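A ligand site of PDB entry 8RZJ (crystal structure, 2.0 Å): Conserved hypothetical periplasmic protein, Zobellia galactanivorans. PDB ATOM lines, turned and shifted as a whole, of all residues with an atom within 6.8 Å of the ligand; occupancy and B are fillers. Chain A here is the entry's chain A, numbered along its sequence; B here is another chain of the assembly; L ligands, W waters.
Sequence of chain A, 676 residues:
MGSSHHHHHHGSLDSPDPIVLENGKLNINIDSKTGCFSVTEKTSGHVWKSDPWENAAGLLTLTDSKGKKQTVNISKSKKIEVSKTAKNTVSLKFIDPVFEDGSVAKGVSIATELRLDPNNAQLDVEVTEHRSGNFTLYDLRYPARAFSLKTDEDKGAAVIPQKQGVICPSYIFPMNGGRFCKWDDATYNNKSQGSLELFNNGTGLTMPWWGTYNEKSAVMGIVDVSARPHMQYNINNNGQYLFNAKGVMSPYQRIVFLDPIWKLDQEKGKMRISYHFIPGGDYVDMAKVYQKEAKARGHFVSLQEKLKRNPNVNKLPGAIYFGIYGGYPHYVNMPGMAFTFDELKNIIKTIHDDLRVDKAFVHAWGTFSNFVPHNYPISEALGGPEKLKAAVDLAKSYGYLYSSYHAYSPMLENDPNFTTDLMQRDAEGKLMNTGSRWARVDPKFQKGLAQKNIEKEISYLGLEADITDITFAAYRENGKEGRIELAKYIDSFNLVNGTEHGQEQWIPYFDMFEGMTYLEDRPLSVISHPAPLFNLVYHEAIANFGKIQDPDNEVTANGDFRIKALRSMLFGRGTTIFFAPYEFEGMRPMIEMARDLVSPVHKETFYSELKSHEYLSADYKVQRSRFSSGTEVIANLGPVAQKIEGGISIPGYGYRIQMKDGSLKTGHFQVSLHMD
The side-chain carboxylate (OD2) of Asp 185 of chain B sits at hydrogen-bond distance from an oxygen (O2) of the ligand. The side-chain carboxylate (OD2) of Asp 469 is in salt-bridge range of a nitrogen (N1) of the ligand (2.8 Å). A ring nitrogen (NE2) of His 330 sits at hydrogen-bond distance from an oxygen (O2) of the ligand. The side-chain carboxylate (OE1) of Glu 500 is in salt-bridge range of a nitrogen (N1) of the ligand, 3.0 Å away.
OD1 of Asp 185 of chain B sits at hydrogen-bond distance from NE2 of His 330. OD1 of Asp 185 of chain B is in hydrogen-bond range of NE1 of Trp 438 (2.9 Å). The side-chain hydroxyl (OH) of Tyr 405 is in hydrogen-bond range of the side-chain carboxylate (OD2) of Asp 469 (2.5 Å). A ring nitrogen (ND1) of His 330 sits at hydrogen-bond distance from the side-chain hydroxyl (OH) of Tyr 325, 2.8 Å away. The side-chain carboxylate (OE1) of Glu 500 sits at hydrogen-bond distance from the backbone NH (N) of Ile 470. NZ of Lys 547 lies within salt-bridge range of OE2 of Glu 500 (2.9 Å). The side-chain amide oxygen of Gln 549 lies within hydrogen-bond range of the side-chain amino group of Lys 547 (2.8 Å).
Merely in contact with the ligand: Trp 365, Tyr 405, Trp 438, Ile 470, Gln 549 and Cys 181 of chain B. Hydrophobic or aromatic side chains within 4 Å of the ligand: His 330, Trp 365, Trp 438 and Ile 470. Ten residues have an atom within 4 Å of the ligand: His 330, Trp 365, Tyr 405, Trp 438, Asp 469, Ile 470, Glu 500, Gln 549, Cys 181 of chain B and Asp 185 of chain B. Along chain A the residues within 4 Å of the ligand span positions 330 to 549.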
ATOM      1  N   TYR A 325     -10.729   5.368  27.801  1.00  0.00           N
ATOM      2  CA  TYR A 325      -9.423   6.012  27.746  1.00  0.00           C
ATOM      3  C   TYR A 325      -9.232   6.890  28.980  1.00  0.00           C
ATOM      4  O   TYR A 325      -9.751   8.001  29.053  1.00  0.00           O
ATOM      5  CB  TYR A 325      -9.261   6.824  26.460  1.00  0.00           C
ATOM      6  CG  TYR A 325      -7.925   7.496  26.426  1.00  0.00           C
ATOM      7  CD1 TYR A 325      -6.772   6.777  26.108  1.00  0.00           C
ATOM      8  CD2 TYR A 325      -7.799   8.834  26.775  1.00  0.00           C
ATOM      9  CE1 TYR A 325      -5.548   7.391  26.115  1.00  0.00           C
ATOM     10  CE2 TYR A 325      -6.560   9.455  26.776  1.00  0.00           C
ATOM     11  CZ  TYR A 325      -5.443   8.739  26.458  1.00  0.00           C
ATOM     12  OH  TYR A 325      -4.205   9.350  26.463  1.00  0.00           O
ATOM     13  N   TYR A 328      -4.098   7.340  29.962  1.00  0.00           N
ATOM     14  CA  TYR A 328      -2.969   6.426  29.966  1.00  0.00           C
ATOM     15  C   TYR A 328      -2.886   5.760  28.598  1.00  0.00           C
ATOM     16  O   TYR A 328      -3.922   5.418  28.027  1.00  0.00           O
ATOM     17  CB  TYR A 328      -3.189   5.387  31.071  1.00  0.00           C
ATOM     18  CG  TYR A 328      -2.061   4.421  31.356  1.00  0.00           C
ATOM     19  CD1 TYR A 328      -1.937   3.230  30.646  1.00  0.00           C
ATOM     20  CD2 TYR A 328      -1.135   4.674  32.373  1.00  0.00           C
ATOM     21  CE1 TYR A 328      -0.918   2.331  30.912  1.00  0.00           C
ATOM     22  CE2 TYR A 328      -0.103   3.764  32.641  1.00  0.00           C
ATOM     23  CZ  TYR A 328      -0.007   2.599  31.910  1.00  0.00           C
ATOM     24  OH  TYR A 328       1.010   1.704  32.159  1.00  0.00           O
ATOM     25  N   PRO A 329      -1.705   5.529  27.999  1.00  0.00           N
ATOM     26  CA  PRO A 329      -0.353   5.580  28.574  1.00  0.00           C
ATOM     27  C   PRO A 329       0.306   6.949  28.681  1.00  0.00           C
ATOM     28  O   PRO A 329       1.412   7.038  29.217  1.00  0.00           O
ATOM     29  CB  PRO A 329       0.447   4.689  27.617  1.00  0.00           C
ATOM     30  CG  PRO A 329      -0.235   4.892  26.291  1.00  0.00           C
ATOM     31  CD  PRO A 329      -1.699   4.977  26.624  1.00  0.00           C
ATOM     32  N   HIS A 330      -0.354   7.980  28.169  1.00  0.00           N
ATOM     33  CA  HIS A 330       0.251   9.306  28.071  1.00  0.00           C
ATOM     34  C   HIS A 330       0.567   9.882  29.443  1.00  0.00           C
ATOM     35  O   HIS A 330       1.573  10.571  29.601  1.00  0.00           O
ATOM     36  CB  HIS A 330      -0.665  10.236  27.276  1.00  0.00           C
ATOM     37  CG  HIS A 330      -0.935   9.736  25.886  1.00  0.00           C
ATOM     38  ND1 HIS A 330      -1.688   8.607  25.629  1.00  0.00           N
ATOM     39  CD2 HIS A 330      -0.507  10.187  24.684  1.00  0.00           C
ATOM     40  CE1 HIS A 330      -1.730   8.397  24.325  1.00  0.00           C
ATOM     41  NE2 HIS A 330      -1.012   9.340  23.728  1.00  0.00           N
ATOM     42  N   TRP A 365      -7.819   1.612  29.296  1.00  0.00           N
ATOM     43  CA  TRP A 365      -6.556   2.336  29.115  1.00  0.00           C
ATOM     44  C   TRP A 365      -6.197   3.071  30.410  1.00  0.00           C
ATOM     45  O   TRP A 365      -6.609   4.213  30.626  1.00  0.00           O
ATOM     46  CB  TRP A 365      -6.646   3.311  27.950  1.00  0.00           C
ATOM     47  CG  TRP A 365      -6.789   2.671  26.591  1.00  0.00           C
ATOM     48  CD1 TRP A 365      -7.654   1.696  26.239  1.00  0.00           C
ATOM     49  CD2 TRP A 365      -6.025   2.980  25.412  1.00  0.00           C
ATOM     50  NE1 TRP A 365      -7.489   1.368  24.907  1.00  0.00           N
ATOM     51  CE2 TRP A 365      -6.496   2.141  24.382  1.00  0.00           C
ATOM     52  CE3 TRP A 365      -4.995   3.888  25.128  1.00  0.00           C
ATOM     53  CZ2 TRP A 365      -5.969   2.171  23.092  1.00  0.00           C
ATOM     54  CZ3 TRP A 365      -4.467   3.927  23.834  1.00  0.00           C
ATOM     55  CH2 TRP A 365      -4.957   3.073  22.838  1.00  0.00           C
ATOM     56  N   TYR A 405      -4.715  -1.857  28.724  1.00  0.00           N
ATOM     57  CA  TYR A 405      -3.762  -1.333  27.749  1.00  0.00           C
ATOM     58  C   TYR A 405      -2.372  -1.872  28.062  1.00  0.00           C
ATOM     59  O   TYR A 405      -1.914  -1.814  29.211  1.00  0.00           O
ATOM     60  CB  TYR A 405      -3.719   0.200  27.777  1.00  0.00           C
ATOM     61  CG  TYR A 405      -2.688   0.765  26.837  1.00  0.00           C
ATOM     62  CD1 TYR A 405      -1.361   0.925  27.231  1.00  0.00           C
ATOM     63  CD2 TYR A 405      -3.031   1.112  25.539  1.00  0.00           C
ATOM     64  CE1 TYR A 405      -0.411   1.423  26.346  1.00  0.00           C
ATOM     65  CE2 TYR A 405      -2.092   1.627  24.665  1.00  0.00           C
ATOM     66  CZ  TYR A 405      -0.794   1.774  25.071  1.00  0.00           C
ATOM     67  OH  TYR A 405       0.118   2.278  24.168  1.00  0.00           O
ATOM     68  N   PRO A 410       7.251   1.834  23.988  1.00  0.00           N
ATOM     69  CA  PRO A 410       7.513   3.248  24.291  1.00  0.00           C
ATOM     70  C   PRO A 410       8.699   3.457  25.213  1.00  0.00           C
ATOM     71  O   PRO A 410       9.112   2.581  25.974  1.00  0.00           O
ATOM     72  CB  PRO A 410       6.216   3.711  24.968  1.00  0.00           C
ATOM     73  CG  PRO A 410       5.193   2.752  24.520  1.00  0.00           C
ATOM     74  CD  PRO A 410       5.920   1.447  24.497  1.00  0.00           C
ATOM     75  N   TRP A 438       6.590   6.564  20.897  1.00  0.00           N
ATOM     76  CA  TRP A 438       5.870   5.332  21.185  1.00  0.00           C
ATOM     77  C   TRP A 438       6.583   4.098  20.673  1.00  0.00           C
ATOM     78  O   TRP A 438       6.200   2.988  21.037  1.00  0.00           O
ATOM     79  CB  TRP A 438       4.444   5.409  20.611  1.00  0.00           C
ATOM     80  CG  TRP A 438       3.692   6.497  21.303  1.00  0.00           C
ATOM     81  CD1 TRP A 438       3.322   7.700  20.795  1.00  0.00           C
ATOM     82  CD2 TRP A 438       3.279   6.498  22.687  1.00  0.00           C
ATOM     83  NE1 TRP A 438       2.683   8.460  21.763  1.00  0.00           N
ATOM     84  CE2 TRP A 438       2.655   7.737  22.927  1.00  0.00           C
ATOM     85  CE3 TRP A 438       3.380   5.576  23.726  1.00  0.00           C
ATOM     86  CZ2 TRP A 438       2.130   8.074  24.179  1.00  0.00           C
ATOM     87  CZ3 TRP A 438       2.853   5.908  24.966  1.00  0.00           C
ATOM     88  CH2 TRP A 438       2.240   7.148  25.186  1.00  0.00           C
ATOM     89  N   ASP A 469      -0.331  -2.678  22.036  1.00  0.00           N
ATOM     90  CA  ASP A 469      -0.237  -1.466  21.247  1.00  0.00           C
ATOM     91  C   ASP A 469       1.079  -1.398  20.460  1.00  0.00           C
ATOM     92  O   ASP A 469       2.086  -2.001  20.847  1.00  0.00           O
ATOM     93  CB  ASP A 469      -0.321  -0.231  22.165  1.00  0.00           C
ATOM     94  CG  ASP A 469      -0.999   0.928  21.493  1.00  0.00           C
ATOM     95  OD1 ASP A 469      -1.884   0.678  20.639  1.00  0.00           O
ATOM     96  OD2 ASP A 469      -0.666   2.092  21.815  1.00  0.00           O
ATOM     97  N   ILE A 470       1.025  -0.683  19.334  1.00  0.00           N
ATOM     98  CA  ILE A 470       2.169  -0.093  18.625  1.00  0.00           C
ATOM     99  C   ILE A 470       3.051  -1.078  17.869  1.00  0.00           C
ATOM    100  O   ILE A 470       3.352  -0.848  16.687  1.00  0.00           O
ATOM    101  CB  ILE A 470       3.059   0.733  19.566  1.00  0.00           C
ATOM    102  CG1 ILE A 470       2.265   1.871  20.214  1.00  0.00           C
ATOM    103  CG2 ILE A 470       4.222   1.347  18.764  1.00  0.00           C
ATOM    104  CD1 ILE A 470       2.857   2.366  21.534  1.00  0.00           C
ATOM    105  N   GLU A 500      -2.702  -2.999  17.651  1.00  0.00           N
ATOM    106  CA  GLU A 500      -2.960  -1.740  16.969  1.00  0.00           C
ATOM    107  C   GLU A 500      -2.592  -1.842  15.496  1.00  0.00           C
ATOM    108  O   GLU A 500      -1.445  -2.168  15.148  1.00  0.00           O
ATOM    109  CB  GLU A 500      -2.180  -0.587  17.610  1.00  0.00           C
ATOM    110  CG  GLU A 500      -2.357   0.725  16.840  1.00  0.00           C
ATOM    111  CD  GLU A 500      -1.486   1.885  17.316  1.00  0.00           C
ATOM    112  OE1 GLU A 500      -0.521   1.675  18.088  1.00  0.00           O
ATOM    113  OE2 GLU A 500      -1.757   3.039  16.892  1.00  0.00           O
ATOM    114  N   GLU A 514      -6.991  -3.468  15.610  1.00  0.00           N
ATOM    115  CA  GLU A 514      -7.673  -2.219  15.936  1.00  0.00           C
ATOM    116  C   GLU A 514      -7.196  -1.170  14.933  1.00  0.00           C
ATOM    117  O   GLU A 514      -6.086  -0.650  15.053  1.00  0.00           O
ATOM    118  CB  GLU A 514      -7.393  -1.798  17.372  1.00  0.00           C
ATOM    119  CG  GLU A 514      -7.805  -0.349  17.686  1.00  0.00           C
ATOM    120  CD  GLU A 514      -6.627   0.609  17.645  1.00  0.00           C
ATOM    121  OE1 GLU A 514      -5.546   0.245  18.166  1.00  0.00           O
ATOM    122  OE2 GLU A 514      -6.770   1.733  17.104  1.00  0.00           O
ATOM    123  N   LYS A 547     -10.252   2.560  14.242  1.00  0.00           N
ATOM    124  CA  LYS A 547      -9.070   3.062  14.933  1.00  0.00           C
ATOM    125  C   LYS A 547      -9.473   3.949  16.115  1.00  0.00           C
ATOM    126  O   LYS A 547     -10.410   4.748  16.014  1.00  0.00           O
ATOM    127  CB  LYS A 547      -8.211   3.855  13.952  1.00  0.00           C
ATOM    128  CG  LYS A 547      -6.814   4.194  14.467  1.00  0.00           C
ATOM    129  CD  LYS A 547      -5.888   2.996  14.307  1.00  0.00           C
ATOM    130  CE  LYS A 547      -4.492   3.258  14.847  1.00  0.00           C
ATOM    131  NZ  LYS A 547      -4.513   3.492  16.319  1.00  0.00           N
ATOM    132  N   ILE A 548      -8.728   3.851  17.218  1.00  0.00           N
ATOM    133  CA  ILE A 548      -9.109   4.576  18.433  1.00  0.00           C
ATOM    134  C   ILE A 548      -9.034   6.095  18.264  1.00  0.00           C
ATOM    135  O   ILE A 548      -9.819   6.826  18.885  1.00  0.00           O
ATOM    136  CB  ILE A 548      -8.290   4.099  19.663  1.00  0.00           C
ATOM    137  CG1 ILE A 548      -6.783   4.376  19.513  1.00  0.00           C
ATOM    138  CG2 ILE A 548      -8.521   2.637  19.930  1.00  0.00           C
ATOM    139  CD1 ILE A 548      -6.307   5.673  20.193  1.00  0.00           C
ATOM    140  N   GLN A 549      -8.107   6.623  17.442  1.00  0.00           N
ATOM    141  CA  GLN A 549      -8.046   8.072  17.258  1.00  0.00           C
ATOM    142  C   GLN A 549      -9.182   8.609  16.395  1.00  0.00           C
ATOM    143  O   GLN A 549      -9.428   9.823  16.387  1.00  0.00           O
ATOM    144  CB  GLN A 549      -6.729   8.508  16.607  1.00  0.00           C
ATOM    145  CG  GLN A 549      -5.488   8.384  17.484  1.00  0.00           C
ATOM    146  CD  GLN A 549      -4.729   7.087  17.239  1.00  0.00           C
ATOM    147  OE1 GLN A 549      -5.319   6.074  16.881  1.00  0.00           O
ATOM    148  NE2 GLN A 549      -3.410   7.118  17.438  1.00  0.00           N
ATOM    149  N   PHE A 578     -14.631   4.845  21.489  1.00  0.00           N
ATOM    150  CA  PHE A 578     -13.424   5.216  22.237  1.00  0.00           C
ATOM    151  C   PHE A 578     -13.666   6.559  22.918  1.00  0.00           C
ATOM    152  O   PHE A 578     -13.804   7.574  22.232  1.00  0.00           O
ATOM    153  CB  PHE A 578     -12.210   5.295  21.304  1.00  0.00           C
ATOM    154  CG  PHE A 578     -10.890   5.227  22.023  1.00  0.00           C
ATOM    155  CD1 PHE A 578     -10.393   4.016  22.466  1.00  0.00           C
ATOM    156  CD2 PHE A 578     -10.126   6.380  22.236  1.00  0.00           C
ATOM    157  CE1 PHE A 578      -9.187   3.940  23.120  1.00  0.00           C
ATOM    158  CE2 PHE A 578      -8.903   6.307  22.900  1.00  0.00           C
ATOM    159  CZ  PHE A 578      -8.433   5.073  23.336  1.00  0.00           C
ATOM    160  N   PHE B 180      -7.450  13.278  22.426  1.00  0.00           N
ATOM    161  CA  PHE B 180      -6.378  13.410  23.398  1.00  0.00           C
ATOM    162  C   PHE B 180      -5.091  12.759  22.888  1.00  0.00           C
ATOM    163  O   PHE B 180      -4.013  13.350  22.962  1.00  0.00           O
ATOM    164  CB  PHE B 180      -6.837  12.785  24.719  1.00  0.00           C
ATOM    165  CG  PHE B 180      -5.918  13.036  25.880  1.00  0.00           C
ATOM    166  CD1 PHE B 180      -4.681  12.392  25.974  1.00  0.00           C
ATOM    167  CD2 PHE B 180      -6.317  13.862  26.923  1.00  0.00           C
ATOM    168  CE1 PHE B 180      -3.850  12.613  27.072  1.00  0.00           C
ATOM    169  CE2 PHE B 180      -5.493  14.090  28.012  1.00  0.00           C
ATOM    170  CZ  PHE B 180      -4.262  13.463  28.093  1.00  0.00           C
ATOM    171  N   CYS B 181      -5.196  11.534  22.377  1.00  0.00           N
ATOM    172  CA  CYS B 181      -4.009  10.857  21.862  1.00  0.00           C
ATOM    173  C   CYS B 181      -3.340  11.678  20.755  1.00  0.00           C
ATOM    174  O   CYS B 181      -2.120  11.865  20.763  1.00  0.00           O
ATOM    175  CB  CYS B 181      -4.385   9.450  21.378  1.00  0.00           C
ATOM    176  SG  CYS B 181      -4.758   8.282  22.704  1.00  0.00           S
ATOM    177  N   LYS B 182      -4.124  12.195  19.798  1.00  0.00           N
ATOM    178  CA  LYS B 182      -3.561  12.976  18.701  1.00  0.00           C
ATOM    179  C   LYS B 182      -2.981  14.291  19.193  1.00  0.00           C
ATOM    180  O   LYS B 182      -1.909  14.726  18.738  1.00  0.00           O
ATOM    181  CB  LYS B 182      -4.635  13.241  17.633  1.00  0.00           C
ATOM    182  CG  LYS B 182      -5.078  11.996  16.830  1.00  0.00           C
ATOM    183  CD  LYS B 182      -6.047  12.345  15.703  1.00  0.00           C
ATOM    184  CE  LYS B 182      -7.414  12.666  16.267  1.00  0.00           C
ATOM    185  NZ  LYS B 182      -8.410  13.054  15.247  1.00  0.00           N
ATOM    186  N   ASP B 184      -1.783  15.140  22.343  1.00  0.00           N
ATOM    187  CA  ASP B 184      -0.550  14.954  23.099  1.00  0.00           C
ATOM    188  C   ASP B 184       0.598  14.496  22.203  1.00  0.00           C
ATOM    189  O   ASP B 184       1.735  14.971  22.351  1.00  0.00           O
ATOM    190  CB  ASP B 184      -0.781  13.949  24.231  1.00  0.00           C
ATOM    191  CG  ASP B 184       0.192  14.109  25.370  1.00  0.00           C
ATOM    192  OD1 ASP B 184       0.178  15.186  26.018  1.00  0.00           O
ATOM    193  OD2 ASP B 184       0.965  13.160  25.642  1.00  0.00           O
ATOM    194  N   ASP B 185       0.319  13.584  21.270  1.00  0.00           N
ATOM    195  CA  ASP B 185       1.375  13.093  20.377  1.00  0.00           C
ATOM    196  C   ASP B 185       1.961  14.215  19.539  1.00  0.00           C
ATOM    197  O   ASP B 185       3.182  14.296  19.332  1.00  0.00           O
ATOM    198  CB  ASP B 185       0.843  11.993  19.463  1.00  0.00           C
ATOM    199  CG  ASP B 185       0.557  10.706  20.216  1.00  0.00           C
ATOM    200  OD1 ASP B 185       0.821  10.661  21.437  1.00  0.00           O
ATOM    201  OD2 ASP B 185       0.061   9.729  19.587  1.00  0.00           O
HETATM  202  C1  LIG L   1       0.040   4.755  19.919  1.00  0.00           C
HETATM  203  C2  LIG L   1      -2.383   4.794  20.095  1.00  0.00           C
HETATM  204  C3  LIG L   1      -2.202   5.886  21.092  1.00  0.00           C
HETATM  205  C4  LIG L   1      -1.241   6.807  20.496  1.00  0.00           C
HETATM  206  C5  LIG L   1      -0.013   5.986  20.808  1.00  0.00           C
HETATM  207  C6  LIG L   1      -0.295   5.532  22.158  1.00  0.00           C
HETATM  208  N1  LIG L   1      -1.189   3.999  19.886  1.00  0.00           N
HETATM  209  O1  LIG L   1      -1.636   5.391  22.253  1.00  0.00           O
HETATM  210  O2  LIG L   1      -1.298   8.056  21.104  1.00  0.00           O
HETATM  211  O   HOH W   1      -3.951   1.997  19.366  1.00  0.00           O
